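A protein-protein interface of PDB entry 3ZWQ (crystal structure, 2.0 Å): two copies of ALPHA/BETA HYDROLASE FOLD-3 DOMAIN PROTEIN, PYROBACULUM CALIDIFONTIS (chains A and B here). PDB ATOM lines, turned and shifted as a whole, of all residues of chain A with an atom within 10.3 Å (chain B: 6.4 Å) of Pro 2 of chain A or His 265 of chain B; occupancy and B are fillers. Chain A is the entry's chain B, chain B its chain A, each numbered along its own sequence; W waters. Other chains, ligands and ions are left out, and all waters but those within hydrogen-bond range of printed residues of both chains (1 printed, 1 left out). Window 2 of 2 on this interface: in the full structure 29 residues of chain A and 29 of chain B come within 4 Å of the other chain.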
ATOM      1  N   MET A   1      -4.875 -27.758 -16.886  1.00  0.00           N
ATOM      2  CA  MET A   1      -5.354 -26.552 -16.162  1.00  0.00           C
ATOM      3  C   MET A   1      -6.813 -26.684 -15.749  1.00  0.00           C
ATOM      4  O   MET A   1      -7.556 -27.446 -16.351  1.00  0.00           O
ATOM      5  CB  MET A   1      -5.268 -25.324 -17.063  1.00  0.00           C
ATOM      6  CG  MET A   1      -3.895 -24.986 -17.620  1.00  0.00           C
ATOM      7  SD  MET A   1      -4.102 -23.533 -18.675  1.00  0.00           S
ATOM      8  CE  MET A   1      -2.427 -22.952 -18.824  1.00  0.00           C
ATOM      9  N   PRO A   2      -7.225 -25.923 -14.720  1.00  0.00           N
ATOM     10  CA  PRO A   2      -8.610 -25.536 -14.518  1.00  0.00           C
ATOM     11  C   PRO A   2      -9.061 -24.574 -15.608  1.00  0.00           C
ATOM     12  O   PRO A   2      -8.268 -24.198 -16.465  1.00  0.00           O
ATOM     13  CB  PRO A   2      -8.578 -24.788 -13.187  1.00  0.00           C
ATOM     14  CG  PRO A   2      -7.388 -25.246 -12.515  1.00  0.00           C
ATOM     15  CD  PRO A   2      -6.394 -25.574 -13.560  1.00  0.00           C
ATOM     16  N   LEU A   3     -10.315 -24.155 -15.547  1.00  0.00           N
ATOM     17  CA  LEU A   3     -10.849 -23.195 -16.498  1.00  0.00           C
ATOM     18  C   LEU A   3     -10.111 -21.868 -16.325  1.00  0.00           C
ATOM     19  O   LEU A   3     -10.014 -21.360 -15.207  1.00  0.00           O
ATOM     20  CB  LEU A   3     -12.350 -23.000 -16.263  1.00  0.00           C
ATOM     21  CG  LEU A   3     -13.252 -22.752 -17.467  1.00  0.00           C
ATOM     22  CD1 LEU A   3     -13.221 -23.951 -18.398  1.00  0.00           C
ATOM     23  CD2 LEU A   3     -14.667 -22.499 -16.981  1.00  0.00           C
ATOM     24  N   SER A   4      -9.581 -21.308 -17.414  1.00  0.00           N
ATOM     25  CA  SER A   4      -8.846 -20.049 -17.311  1.00  0.00           C
ATOM     26  C   SER A   4      -9.751 -18.988 -16.663  1.00  0.00           C
ATOM     27  O   SER A   4     -10.946 -18.952 -16.943  1.00  0.00           O
ATOM     28  CB  SER A   4      -8.322 -19.566 -18.677  1.00  0.00           C
ATOM     29  OG  SER A   4      -9.286 -18.786 -19.369  1.00  0.00           O
ATOM     30  N   PRO A   5      -9.188 -18.147 -15.778  1.00  0.00           N
ATOM     31  CA  PRO A   5     -10.001 -17.184 -15.017  1.00  0.00           C
ATOM     32  C   PRO A   5     -10.935 -16.298 -15.858  1.00  0.00           C
ATOM     33  O   PRO A   5     -12.113 -16.193 -15.529  1.00  0.00           O
ATOM     34  CB  PRO A   5      -8.956 -16.336 -14.289  1.00  0.00           C
ATOM     35  CG  PRO A   5      -7.777 -17.241 -14.134  1.00  0.00           C
ATOM     36  CD  PRO A   5      -7.776 -18.143 -15.342  1.00  0.00           C
ATOM     37  N   ILE A   6     -10.443 -15.690 -16.939  1.00  0.00           N
ATOM     38  CA  ILE A   6     -11.302 -14.806 -17.754  1.00  0.00           C
ATOM     39  C   ILE A   6     -12.504 -15.562 -18.342  1.00  0.00           C
ATOM     40  O   ILE A   6     -13.605 -15.018 -18.443  1.00  0.00           O
ATOM     41  CB  ILE A   6     -10.506 -14.057 -18.872  1.00  0.00           C
ATOM     42  CG1 ILE A   6     -11.300 -12.844 -19.396  1.00  0.00           C
ATOM     43  CG2 ILE A   6     -10.150 -14.985 -20.025  1.00  0.00           C
ATOM     44  CD1 ILE A   6     -11.461 -11.710 -18.388  1.00  0.00           C
ATOM     45  N   LEU A   7     -12.296 -16.830 -18.681  1.00  0.00           N
ATOM     46  CA  LEU A   7     -13.344 -17.665 -19.261  1.00  0.00           C
ATOM     47  C   LEU A   7     -14.453 -18.008 -18.258  1.00  0.00           C
ATOM     48  O   LEU A   7     -15.619 -18.138 -18.641  1.00  0.00           O
ATOM     49  CB  LEU A   7     -12.730 -18.950 -19.832  1.00  0.00           C
ATOM     50  CG  LEU A   7     -13.418 -19.553 -21.051  1.00  0.00           C
ATOM     51  CD1 LEU A   7     -13.547 -18.526 -22.166  1.00  0.00           C
ATOM     52  CD2 LEU A   7     -12.636 -20.775 -21.523  1.00  0.00           C
ATOM     53  N   ARG A   8     -14.099 -18.167 -16.983  1.00  0.00           N
ATOM     54  CA  ARG A   8     -15.113 -18.346 -15.938  1.00  0.00           C
ATOM     55  C   ARG A   8     -15.972 -17.095 -15.866  1.00  0.00           C
ATOM     56  O   ARG A   8     -17.197 -17.171 -15.885  1.00  0.00           O
ATOM     57  CB  ARG A   8     -14.470 -18.595 -14.573  1.00  0.00           C
ATOM     58  CG  ARG A   8     -13.780 -19.931 -14.441  1.00  0.00           C
ATOM     59  CD  ARG A   8     -12.995 -20.007 -13.142  1.00  0.00           C
ATOM     60  NE  ARG A   8     -13.867 -19.975 -11.965  1.00  0.00           N
ATOM     61  CZ  ARG A   8     -14.033 -20.976 -11.095  1.00  0.00           C
ATOM     62  NH1 ARG A   8     -13.382 -22.134 -11.232  1.00  0.00           N
ATOM     63  NH2 ARG A   8     -14.857 -20.817 -10.063  1.00  0.00           N
ATOM     64  N   LEU A  11     -18.312 -16.933 -18.863  1.00  0.00           N
ATOM     65  CA  LEU A  11     -19.396 -17.900 -18.686  1.00  0.00           C
ATOM     66  C   LEU A  11     -20.419 -17.427 -17.650  1.00  0.00           C
ATOM     67  O   LEU A  11     -21.626 -17.498 -17.891  1.00  0.00           O
ATOM     68  CB  LEU A  11     -18.840 -19.273 -18.292  1.00  0.00           C
ATOM     69  CG  LEU A  11     -18.208 -20.069 -19.440  1.00  0.00           C
ATOM     70  CD1 LEU A  11     -17.331 -21.186 -18.913  1.00  0.00           C
ATOM     71  CD2 LEU A  11     -19.292 -20.620 -20.350  1.00  0.00           C
ATOM     72  N   TYR A 201     -18.431 -32.798 -19.981  1.00  0.00           N
ATOM     73  CA  TYR A 201     -18.363 -31.353 -20.252  1.00  0.00           C
ATOM     74  C   TYR A 201     -19.594 -30.797 -20.971  1.00  0.00           C
ATOM     75  O   TYR A 201     -19.507 -29.754 -21.609  1.00  0.00           O
ATOM     76  CB  TYR A 201     -17.096 -31.053 -21.068  1.00  0.00           C
ATOM     77  CG  TYR A 201     -15.875 -31.716 -20.477  1.00  0.00           C
ATOM     78  CD1 TYR A 201     -15.413 -31.342 -19.232  1.00  0.00           C
ATOM     79  CD2 TYR A 201     -15.211 -32.747 -21.150  1.00  0.00           C
ATOM     80  CE1 TYR A 201     -14.317 -31.938 -18.671  1.00  0.00           C
ATOM     81  CE2 TYR A 201     -14.110 -33.365 -20.586  1.00  0.00           C
ATOM     82  CZ  TYR A 201     -13.664 -32.954 -19.348  1.00  0.00           C
ATOM     83  OH  TYR A 201     -12.574 -33.553 -18.752  1.00  0.00           O
ATOM     84  N   TYR A 206     -21.700 -25.333 -18.545  1.00  0.00           N
ATOM     85  CA  TYR A 206     -20.776 -25.050 -19.661  1.00  0.00           C
ATOM     86  C   TYR A 206     -21.365 -24.152 -20.750  1.00  0.00           C
ATOM     87  O   TYR A 206     -20.610 -23.490 -21.469  1.00  0.00           O
ATOM     88  CB  TYR A 206     -20.253 -26.354 -20.276  1.00  0.00           C
ATOM     89  CG  TYR A 206     -19.190 -26.989 -19.418  1.00  0.00           C
ATOM     90  CD1 TYR A 206     -17.927 -26.430 -19.337  1.00  0.00           C
ATOM     91  CD2 TYR A 206     -19.460 -28.120 -18.646  1.00  0.00           C
ATOM     92  CE1 TYR A 206     -16.954 -26.975 -18.538  1.00  0.00           C
ATOM     93  CE2 TYR A 206     -18.478 -28.680 -17.839  1.00  0.00           C
ATOM     94  CZ  TYR A 206     -17.225 -28.099 -17.802  1.00  0.00           C
ATOM     95  OH  TYR A 206     -16.236 -28.621 -17.016  1.00  0.00           O
ATOM     96  N   ALA A 251     -10.037 -28.869 -27.288  1.00  0.00           N
ATOM     97  CA  ALA A 251     -10.138 -28.109 -26.044  1.00  0.00           C
ATOM     98  C   ALA A 251     -10.281 -29.045 -24.835  1.00  0.00           C
ATOM     99  O   ALA A 251     -10.940 -30.071 -24.908  1.00  0.00           O
ATOM    100  CB  ALA A 251     -11.334 -27.143 -26.096  1.00  0.00           C
ATOM    101  N   GLU A 252      -9.690 -28.670 -23.709  1.00  0.00           N
ATOM    102  CA  GLU A 252      -9.700 -29.546 -22.542  1.00  0.00           C
ATOM    103  C   GLU A 252     -11.145 -29.792 -22.033  1.00  0.00           C
ATOM    104  O   GLU A 252     -11.524 -30.938 -21.767  1.00  0.00           O
ATOM    105  CB  GLU A 252      -8.826 -28.971 -21.429  1.00  0.00           C
ATOM    106  CG  GLU A 252      -8.896 -29.758 -20.122  1.00  0.00           C
ATOM    107  CD  GLU A 252      -7.963 -29.252 -19.076  1.00  0.00           C
ATOM    108  OE1 GLU A 252      -7.504 -28.099 -19.184  1.00  0.00           O
ATOM    109  OE2 GLU A 252      -7.699 -30.000 -18.111  1.00  0.00           O
ATOM    110  N   TYR A 253     -11.941 -28.728 -21.932  1.00  0.00           N
ATOM    111  CA  TYR A 253     -13.308 -28.833 -21.396  1.00  0.00           C
ATOM    112  C   TYR A 253     -14.318 -28.836 -22.497  1.00  0.00           C
ATOM    113  O   TYR A 253     -15.106 -27.901 -22.649  1.00  0.00           O
ATOM    114  CB  TYR A 253     -13.582 -27.694 -20.436  1.00  0.00           C
ATOM    115  CG  TYR A 253     -12.628 -27.721 -19.288  1.00  0.00           C
ATOM    116  CD1 TYR A 253     -12.807 -28.599 -18.226  1.00  0.00           C
ATOM    117  CD2 TYR A 253     -11.520 -26.898 -19.275  1.00  0.00           C
ATOM    118  CE1 TYR A 253     -11.900 -28.631 -17.160  1.00  0.00           C
ATOM    119  CE2 TYR A 253     -10.628 -26.919 -18.237  1.00  0.00           C
ATOM    120  CZ  TYR A 253     -10.814 -27.783 -17.187  1.00  0.00           C
ATOM    121  OH  TYR A 253      -9.897 -27.783 -16.170  1.00  0.00           O
ATOM    122  N   TYR A 279      -5.565 -27.908 -26.153  1.00  0.00           N
ATOM    123  CA  TYR A 279      -5.444 -26.623 -25.450  1.00  0.00           C
ATOM    124  C   TYR A 279      -6.096 -26.754 -24.077  1.00  0.00           C
ATOM    125  O   TYR A 279      -7.284 -27.046 -23.966  1.00  0.00           O
ATOM    126  CB  TYR A 279      -6.073 -25.471 -26.268  1.00  0.00           C
ATOM    127  CG  TYR A 279      -5.136 -24.976 -27.381  1.00  0.00           C
ATOM    128  CD1 TYR A 279      -4.780 -25.812 -28.445  1.00  0.00           C
ATOM    129  CD2 TYR A 279      -4.560 -23.704 -27.324  1.00  0.00           C
ATOM    130  CE1 TYR A 279      -3.903 -25.379 -29.450  1.00  0.00           C
ATOM    131  CE2 TYR A 279      -3.679 -23.251 -28.330  1.00  0.00           C
ATOM    132  CZ  TYR A 279      -3.352 -24.097 -29.383  1.00  0.00           C
ATOM    133  OH  TYR A 279      -2.473 -23.658 -30.357  1.00  0.00           O
ATOM    134  N   ASN A 280      -5.294 -26.580 -23.033  1.00  0.00           N
ATOM    135  CA  ASN A 280      -5.779 -26.648 -21.671  1.00  0.00           C
ATOM    136  C   ASN A 280      -6.514 -25.382 -21.259  1.00  0.00           C
ATOM    137  O   ASN A 280      -6.237 -24.290 -21.777  1.00  0.00           O
ATOM    138  CB  ASN A 280      -4.618 -26.899 -20.722  1.00  0.00           C
ATOM    139  CG  ASN A 280      -4.053 -28.321 -20.846  1.00  0.00           C
ATOM    140  OD1 ASN A 280      -4.752 -29.245 -21.238  1.00  0.00           O
ATOM    141  ND2 ASN A 280      -2.773 -28.481 -20.537  1.00  0.00           N
ATOM    142  N   GLY A 281      -7.460 -25.541 -20.338  1.00  0.00           N
ATOM    143  CA  GLY A 281      -8.071 -24.409 -19.651  1.00  0.00           C
ATOM    144  C   GLY A 281      -9.200 -23.723 -20.387  1.00  0.00           C
ATOM    145  O   GLY A 281      -9.665 -22.661 -19.961  1.00  0.00           O
ATOM    146  N   VAL A 282      -9.668 -24.338 -21.465  1.00  0.00           N
ATOM    147  CA  VAL A 282     -10.571 -23.681 -22.377  1.00  0.00           C
ATOM    148  C   VAL A 282     -11.648 -24.635 -22.824  1.00  0.00           C
ATOM    149  O   VAL A 282     -11.527 -25.849 -22.655  1.00  0.00           O
ATOM    150  CB  VAL A 282      -9.829 -23.107 -23.616  1.00  0.00           C
ATOM    151  CG1 VAL A 282      -8.976 -21.920 -23.190  1.00  0.00           C
ATOM    152  CG2 VAL A 282      -8.994 -24.193 -24.317  1.00  0.00           C
ATOM    153  N   ILE A 283     -12.704 -24.052 -23.370  1.00  0.00           N
ATOM    154  CA  ILE A 283     -13.899 -24.769 -23.770  1.00  0.00           C
ATOM    155  C   ILE A 283     -14.021 -24.854 -25.285  1.00  0.00           C
ATOM    156  O   ILE A 283     -13.252 -24.239 -26.041  1.00  0.00           O
ATOM    157  CB  ILE A 283     -15.176 -24.079 -23.203  1.00  0.00           C
ATOM    158  CG1 ILE A 283     -15.288 -22.619 -23.691  1.00  0.00           C
ATOM    159  CG2 ILE A 283     -15.160 -24.139 -21.688  1.00  0.00           C
ATOM    160  CD1 ILE A 283     -16.605 -21.939 -23.328  1.00  0.00           C
ATOM    161  N   LEU A 293      -8.858 -13.953 -25.260  1.00  0.00           N
ATOM    162  CA  LEU A 293      -8.332 -15.237 -24.787  1.00  0.00           C
ATOM    163  C   LEU A 293      -6.991 -15.551 -25.471  1.00  0.00           C
ATOM    164  O   LEU A 293      -6.955 -15.753 -26.679  1.00  0.00           O
ATOM    165  CB  LEU A 293      -9.333 -16.335 -25.143  1.00  0.00           C
ATOM    166  CG  LEU A 293      -9.443 -17.534 -24.222  1.00  0.00           C
ATOM    167  CD1 LEU A 293     -10.060 -17.101 -22.901  1.00  0.00           C
ATOM    168  CD2 LEU A 293     -10.306 -18.593 -24.893  1.00  0.00           C
ATOM    169  N   GLU A 294      -5.900 -15.600 -24.704  1.00  0.00           N
ATOM    170  CA  GLU A 294      -4.570 -15.884 -25.282  1.00  0.00           C
ATOM    171  C   GLU A 294      -4.533 -17.244 -25.978  1.00  0.00           C
ATOM    172  O   GLU A 294      -3.816 -17.404 -26.947  1.00  0.00           O
ATOM    173  CB  GLU A 294      -3.448 -15.778 -24.232  1.00  0.00           C
ATOM    174  CG  GLU A 294      -3.635 -16.635 -22.976  1.00  0.00           C
ATOM    175  CD  GLU A 294      -4.278 -15.866 -21.821  1.00  0.00           C
ATOM    176  OE1 GLU A 294      -5.300 -15.175 -22.076  1.00  0.00           O
ATOM    177  OE2 GLU A 294      -3.752 -15.951 -20.681  1.00  0.00           O
ATOM    178  N   GLU A 295      -5.331 -18.211 -25.498  1.00  0.00           N
ATOM    179  CA  GLU A 295      -5.411 -19.553 -26.102  1.00  0.00           C
ATOM    180  C   GLU A 295      -5.947 -19.453 -27.510  1.00  0.00           C
ATOM    181  O   GLU A 295      -5.511 -20.191 -28.392  1.00  0.00           O
ATOM    182  CB  GLU A 295      -6.305 -20.518 -25.293  1.00  0.00           C
ATOM    183  CG  GLU A 295      -5.711 -21.056 -23.986  1.00  0.00           C
ATOM    184  CD  GLU A 295      -5.766 -20.061 -22.863  1.00  0.00           C
ATOM    185  OE1 GLU A 295      -6.373 -18.974 -23.043  1.00  0.00           O
ATOM    186  OE2 GLU A 295      -5.182 -20.341 -21.798  1.00  0.00           O
ATOM    187  N   GLY B 260       4.170 -28.930 -15.741  1.00  0.00           N
ATOM    188  CA  GLY B 260       4.182 -27.964 -16.817  1.00  0.00           C
ATOM    189  C   GLY B 260       2.836 -27.291 -16.945  1.00  0.00           C
ATOM    190  O   GLY B 260       2.739 -26.077 -17.071  1.00  0.00           O
ATOM    191  N   GLU B 261       1.788 -28.097 -16.901  1.00  0.00           N
ATOM    192  CA  GLU B 261       0.441 -27.581 -16.979  1.00  0.00           C
ATOM    193  C   GLU B 261       0.091 -26.776 -15.730  1.00  0.00           C
ATOM    194  O   GLU B 261      -0.545 -25.726 -15.818  1.00  0.00           O
ATOM    195  CB  GLU B 261      -0.522 -28.726 -17.260  1.00  0.00           C
ATOM    196  CG  GLU B 261      -0.124 -29.406 -18.571  1.00  0.00           C
ATOM    197  CD  GLU B 261      -1.045 -30.515 -18.998  1.00  0.00           C
ATOM    198  OE1 GLU B 261      -1.950 -30.867 -18.212  1.00  0.00           O
ATOM    199  OE2 GLU B 261      -0.828 -31.042 -20.127  1.00  0.00           O
ATOM    200  N   LEU B 262       0.570 -27.216 -14.581  1.00  0.00           N
ATOM    201  CA  LEU B 262       0.383 -26.436 -13.360  1.00  0.00           C
ATOM    202  C   LEU B 262       1.083 -25.067 -13.437  1.00  0.00           C
ATOM    203  O   LEU B 262       0.526 -24.066 -12.969  1.00  0.00           O
ATOM    204  CB  LEU B 262       0.835 -27.218 -12.130  1.00  0.00           C
ATOM    205  CG  LEU B 262      -0.110 -28.365 -11.751  1.00  0.00           C
ATOM    206  CD1 LEU B 262       0.599 -29.420 -10.911  1.00  0.00           C
ATOM    207  CD2 LEU B 262      -1.332 -27.822 -11.016  1.00  0.00           C
ATOM    208  N   TYR B 263       2.278 -25.018 -14.045  1.00  0.00           N
ATOM    209  CA  TYR B 263       3.023 -23.774 -14.153  1.00  0.00           C
ATOM    210  C   TYR B 263       2.258 -22.742 -14.981  1.00  0.00           C
ATOM    211  O   TYR B 263       2.169 -21.586 -14.599  1.00  0.00           O
ATOM    212  CB  TYR B 263       4.375 -24.011 -14.798  1.00  0.00           C
ATOM    213  CG  TYR B 263       5.327 -22.859 -14.619  1.00  0.00           C
ATOM    214  CD1 TYR B 263       5.826 -22.558 -13.372  1.00  0.00           C
ATOM    215  CD2 TYR B 263       5.735 -22.073 -15.702  1.00  0.00           C
ATOM    216  CE1 TYR B 263       6.700 -21.536 -13.194  1.00  0.00           C
ATOM    217  CE2 TYR B 263       6.624 -21.036 -15.532  1.00  0.00           C
ATOM    218  CZ  TYR B 263       7.100 -20.768 -14.285  1.00  0.00           C
ATOM    219  OH  TYR B 263       7.995 -19.755 -14.079  1.00  0.00           O
ATOM    220  N   ALA B 264       1.716 -23.192 -16.110  1.00  0.00           N
ATOM    221  CA  ALA B 264       0.881 -22.375 -16.973  1.00  0.00           C
ATOM    222  C   ALA B 264      -0.317 -21.801 -16.226  1.00  0.00           C
ATOM    223  O   ALA B 264      -0.620 -20.597 -16.351  1.00  0.00           O
ATOM    224  CB  ALA B 264       0.403 -23.203 -18.180  1.00  0.00           C
ATOM    225  N   HIS B 265      -1.007 -22.651 -15.455  1.00  0.00           N
ATOM    226  CA  HIS B 265      -2.158 -22.200 -14.695  1.00  0.00           C
ATOM    227  C   HIS B 265      -1.774 -21.173 -13.637  1.00  0.00           C
ATOM    228  O   HIS B 265      -2.440 -20.150 -13.499  1.00  0.00           O
ATOM    229  CB  HIS B 265      -2.916 -23.352 -14.040  1.00  0.00           C
ATOM    230  CG  HIS B 265      -3.856 -22.901 -12.968  1.00  0.00           C
ATOM    231  ND1 HIS B 265      -5.140 -22.480 -13.238  1.00  0.00           N
ATOM    232  CD2 HIS B 265      -3.680 -22.755 -11.635  1.00  0.00           C
ATOM    233  CE1 HIS B 265      -5.728 -22.130 -12.107  1.00  0.00           C
ATOM    234  NE2 HIS B 265      -4.864 -22.294 -11.119  1.00  0.00           N
ATOM    235  N   LEU B 266      -0.716 -21.453 -12.892  1.00  0.00           N
ATOM    236  CA  LEU B 266      -0.266 -20.552 -11.859  1.00  0.00           C
ATOM    237  C   LEU B 266       0.185 -19.180 -12.422  1.00  0.00           C
ATOM    238  O   LEU B 266      -0.078 -18.150 -11.825  1.00  0.00           O
ATOM    239  CB  LEU B 266       0.837 -21.217 -11.029  1.00  0.00           C
ATOM    240  CG  LEU B 266       0.339 -22.381 -10.148  1.00  0.00           C
ATOM    241  CD1 LEU B 266       1.509 -23.212  -9.648  1.00  0.00           C
ATOM    242  CD2 LEU B 266      -0.529 -21.866  -8.962  1.00  0.00           C
ATOM    243  N   LEU B 267       0.864 -19.183 -13.565  1.00  0.00           N
ATOM    244  CA  LEU B 267       1.140 -17.948 -14.278  1.00  0.00           C
ATOM    245  C   LEU B 267      -0.154 -17.125 -14.459  1.00  0.00           C
ATOM    246  O   LEU B 267      -0.196 -15.944 -14.120  1.00  0.00           O
ATOM    247  CB  LEU B 267       1.790 -18.251 -15.627  1.00  0.00           C
ATOM    248  CG  LEU B 267       3.268 -18.643 -15.635  1.00  0.00           C
ATOM    249  CD1 LEU B 267       3.613 -19.193 -17.005  1.00  0.00           C
ATOM    250  CD2 LEU B 267       4.136 -17.439 -15.280  1.00  0.00           C
ATOM    251  N   LYS B 268      -1.203 -17.755 -14.977  1.00  0.00           N
ATOM    252  CA  LYS B 268      -2.504 -17.086 -15.155  1.00  0.00           C
ATOM    253  C   LYS B 268      -3.078 -16.474 -13.869  1.00  0.00           C
ATOM    254  O   LYS B 268      -3.655 -15.381 -13.900  1.00  0.00           O
ATOM    255  CB  LYS B 268      -3.548 -18.051 -15.702  1.00  0.00           C
ATOM    256  CG  LYS B 268      -3.275 -18.600 -17.080  1.00  0.00           C
ATOM    257  CD  LYS B 268      -4.389 -19.603 -17.429  1.00  0.00           C
ATOM    258  CE  LYS B 268      -4.317 -20.025 -18.884  1.00  0.00           C
ATOM    259  NZ  LYS B 268      -4.672 -18.898 -19.814  1.00  0.00           N
ATOM    260  N   THR B 269      -2.928 -17.172 -12.748  1.00  0.00           N
ATOM    261  CA  THR B 269      -3.532 -16.732 -11.501  1.00  0.00           C
ATOM    262  C   THR B 269      -2.885 -15.435 -11.025  1.00  0.00           C
ATOM    263  O   THR B 269      -3.480 -14.707 -10.262  1.00  0.00           O
ATOM    264  CB  THR B 269      -3.426 -17.809 -10.402  1.00  0.00           C
ATOM    265  OG1 THR B 269      -2.065 -17.942  -9.991  1.00  0.00           O
ATOM    266  CG2 THR B 269      -3.927 -19.163 -10.920  1.00  0.00           C
ATOM    267  N   ARG B 270      -1.665 -15.161 -11.493  1.00  0.00           N
ATOM    268  CA  ARG B 270      -0.963 -13.926 -11.163  1.00  0.00           C
ATOM    269  C   ARG B 270      -1.040 -12.937 -12.326  1.00  0.00           C
ATOM    270  O   ARG B 270      -0.302 -11.948 -12.369  1.00  0.00           O
ATOM    271  CB  ARG B 270       0.500 -14.226 -10.824  1.00  0.00           C
ATOM    272  CG  ARG B 270       0.701 -15.276  -9.745  1.00  0.00           C
ATOM    273  CD  ARG B 270      -0.044 -14.941  -8.444  1.00  0.00           C
ATOM    274  NE  ARG B 270       0.107 -13.535  -8.076  1.00  0.00           N
ATOM    275  CZ  ARG B 270       1.146 -13.025  -7.422  1.00  0.00           C
ATOM    276  NH1 ARG B 270       2.169 -13.787  -7.051  1.00  0.00           N
ATOM    277  NH2 ARG B 270       1.172 -11.733  -7.140  1.00  0.00           N
ATOM    278  N   ALA B 274      -0.641 -16.708 -20.649  1.00  0.00           N
ATOM    279  CA  ALA B 274      -0.004 -18.017 -20.591  1.00  0.00           C
ATOM    280  C   ALA B 274      -0.908 -19.048 -21.253  1.00  0.00           C
ATOM    281  O   ALA B 274      -2.103 -19.080 -20.983  1.00  0.00           O
ATOM    282  CB  ALA B 274       0.262 -18.394 -19.141  1.00  0.00           C
ATOM    283  N   ALA B 276      -1.012 -23.331 -22.250  1.00  0.00           N
ATOM    284  CA  ALA B 276      -0.481 -24.686 -22.141  1.00  0.00           C
ATOM    285  C   ALA B 276      -1.177 -25.543 -23.174  1.00  0.00           C
ATOM    286  O   ALA B 276      -2.417 -25.591 -23.214  1.00  0.00           O
ATOM    287  CB  ALA B 276      -0.724 -25.277 -20.713  1.00  0.00           C
HETATM  288  O   HOH W   1      -7.232 -17.535 -20.915  1.00  0.00           O
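Water W1 lies within hydrogen-bond range of the side-chain carboxylate of Glu 295 of chain A, the side-chain hydroxyl of Ser 4 of chain A, the side-chain amino group of Lys 268 of chain B and the side-chain carboxylate of Glu 294 of chain A.
OE2 of Glu 261 of chain B lies close to ND2 of Asn 280 of chain A.
The side-chain amino group of Lys 268 of chain B lies within salt-bridge range of the side-chain carboxylate of Glu 294 of chain A (3.2 Å).
The side-chain amino group of Lys 268 of chain B is in salt-bridge range of the side-chain carboxylate of Glu 295 of chain A (2.5 Å).
N of Ala 274 of chain B lies within hydrogen-bond range of OE2 of Glu 294 of chain A, 3.2 Å away.
The backbone NH (N) of Asn 280 of chain A sits at hydrogen-bond distance from the backbone carbonyl oxygen (O) of Ala 276 of chain B (3.0 Å).
The backbone carbonyl oxygen of Ala 274 of chain B sits close to the side-chain carboxylate of Glu 295 of chain A (3.4 Å).
No position is printed for both chains.
Of the 14 pairs that touch across the chains among the printed residues, none has its exchanged pair printed and touching as well.
The side-chain amino group (NZ) of Lys 268 of chain B lies within hydrogen-bond range of the backbone carbonyl oxygen (O) of Ala 274 of chain B (2.8 Å).
O of Gly 281 of chain A lies within hydrogen-bond range of N of Ser 4 of chain A (2.9 Å).
The backbone NH (N) of Glu 252 of chain A lies within hydrogen-bond range of the backbone carbonyl oxygen (O) of Tyr 279 of chain A (2.9 Å).
Of the printed residues of chain B, Met 1 of chain A touches Glu 261 (3.9 Å), Ala 264 (2.9 Å), His 265 (3.7 Å), Lys 268 (3.5 Å) and Ala 276 (3.4 Å).
Printed residues of chain B within 4 Å of Pro 2 of chain A: His 265.
Tyr 206 of chain A touches none of the printed residues of chain B.
Printed residues of chain B within 4 Å of Tyr 279 of chain A: Ala 276 (3.9 Å).
Printed residues of chain B within 4 Å of Asn 280 of chain A: Glu 261 and Ala 276.
Of chain A, only Met 1 comes within 4 Å of Ala 264 of chain B.
His 265 of chain B touches two residues of chain A.
No residue of chain A comes within 4 Å of Leu 266 of chain B.
Of the printed residues of chain A, Lys 268 of chain B touches Met 1, Ser 4, Glu 294 and Glu 295.
Printed residues of chain A within 4 Å of Ala 276 of chain B: Met 1, Tyr 279 and Asn 280.
The nearest printed residue of chain B that does not touch Ser 4 of chain A is His 265 of chain B (6.0 Å).
Among the printed residues, merely in contact across the chains: Met 1 of chain A with Ala 264 of chain B (2.9 Å), Pro 2 of chain A with His 265 of chain B (3.4 Å), Met 1 of chain A with Ala 276 of chain B (3.4 Å), Met 1 of chain A with Lys 268 of chain B (3.5 Å), Met 1 of chain A with His 265 of chain B (3.7 Å), Met 1 of chain A with Glu 261 of chain B (3.9 Å), Ser 4 of chain A with Lys 268 of chain B (3.9 Å) and Tyr 279 of chain A with Ala 276 of chain B (3.9 Å).
Of the 22 printed residues of chain A, 7 touch a printed residue of chain B.
Hydrophobic or aromatic side chains of chain A that line the printed part of chain B: Met 1 and Pro 2.
Hydrophobic or aromatic side chains of chain B within 4 Å of the printed part of chain A: Ala 264, His 265 and Ala 276.
Among the printed residues, 14 pairs touch across the chains.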
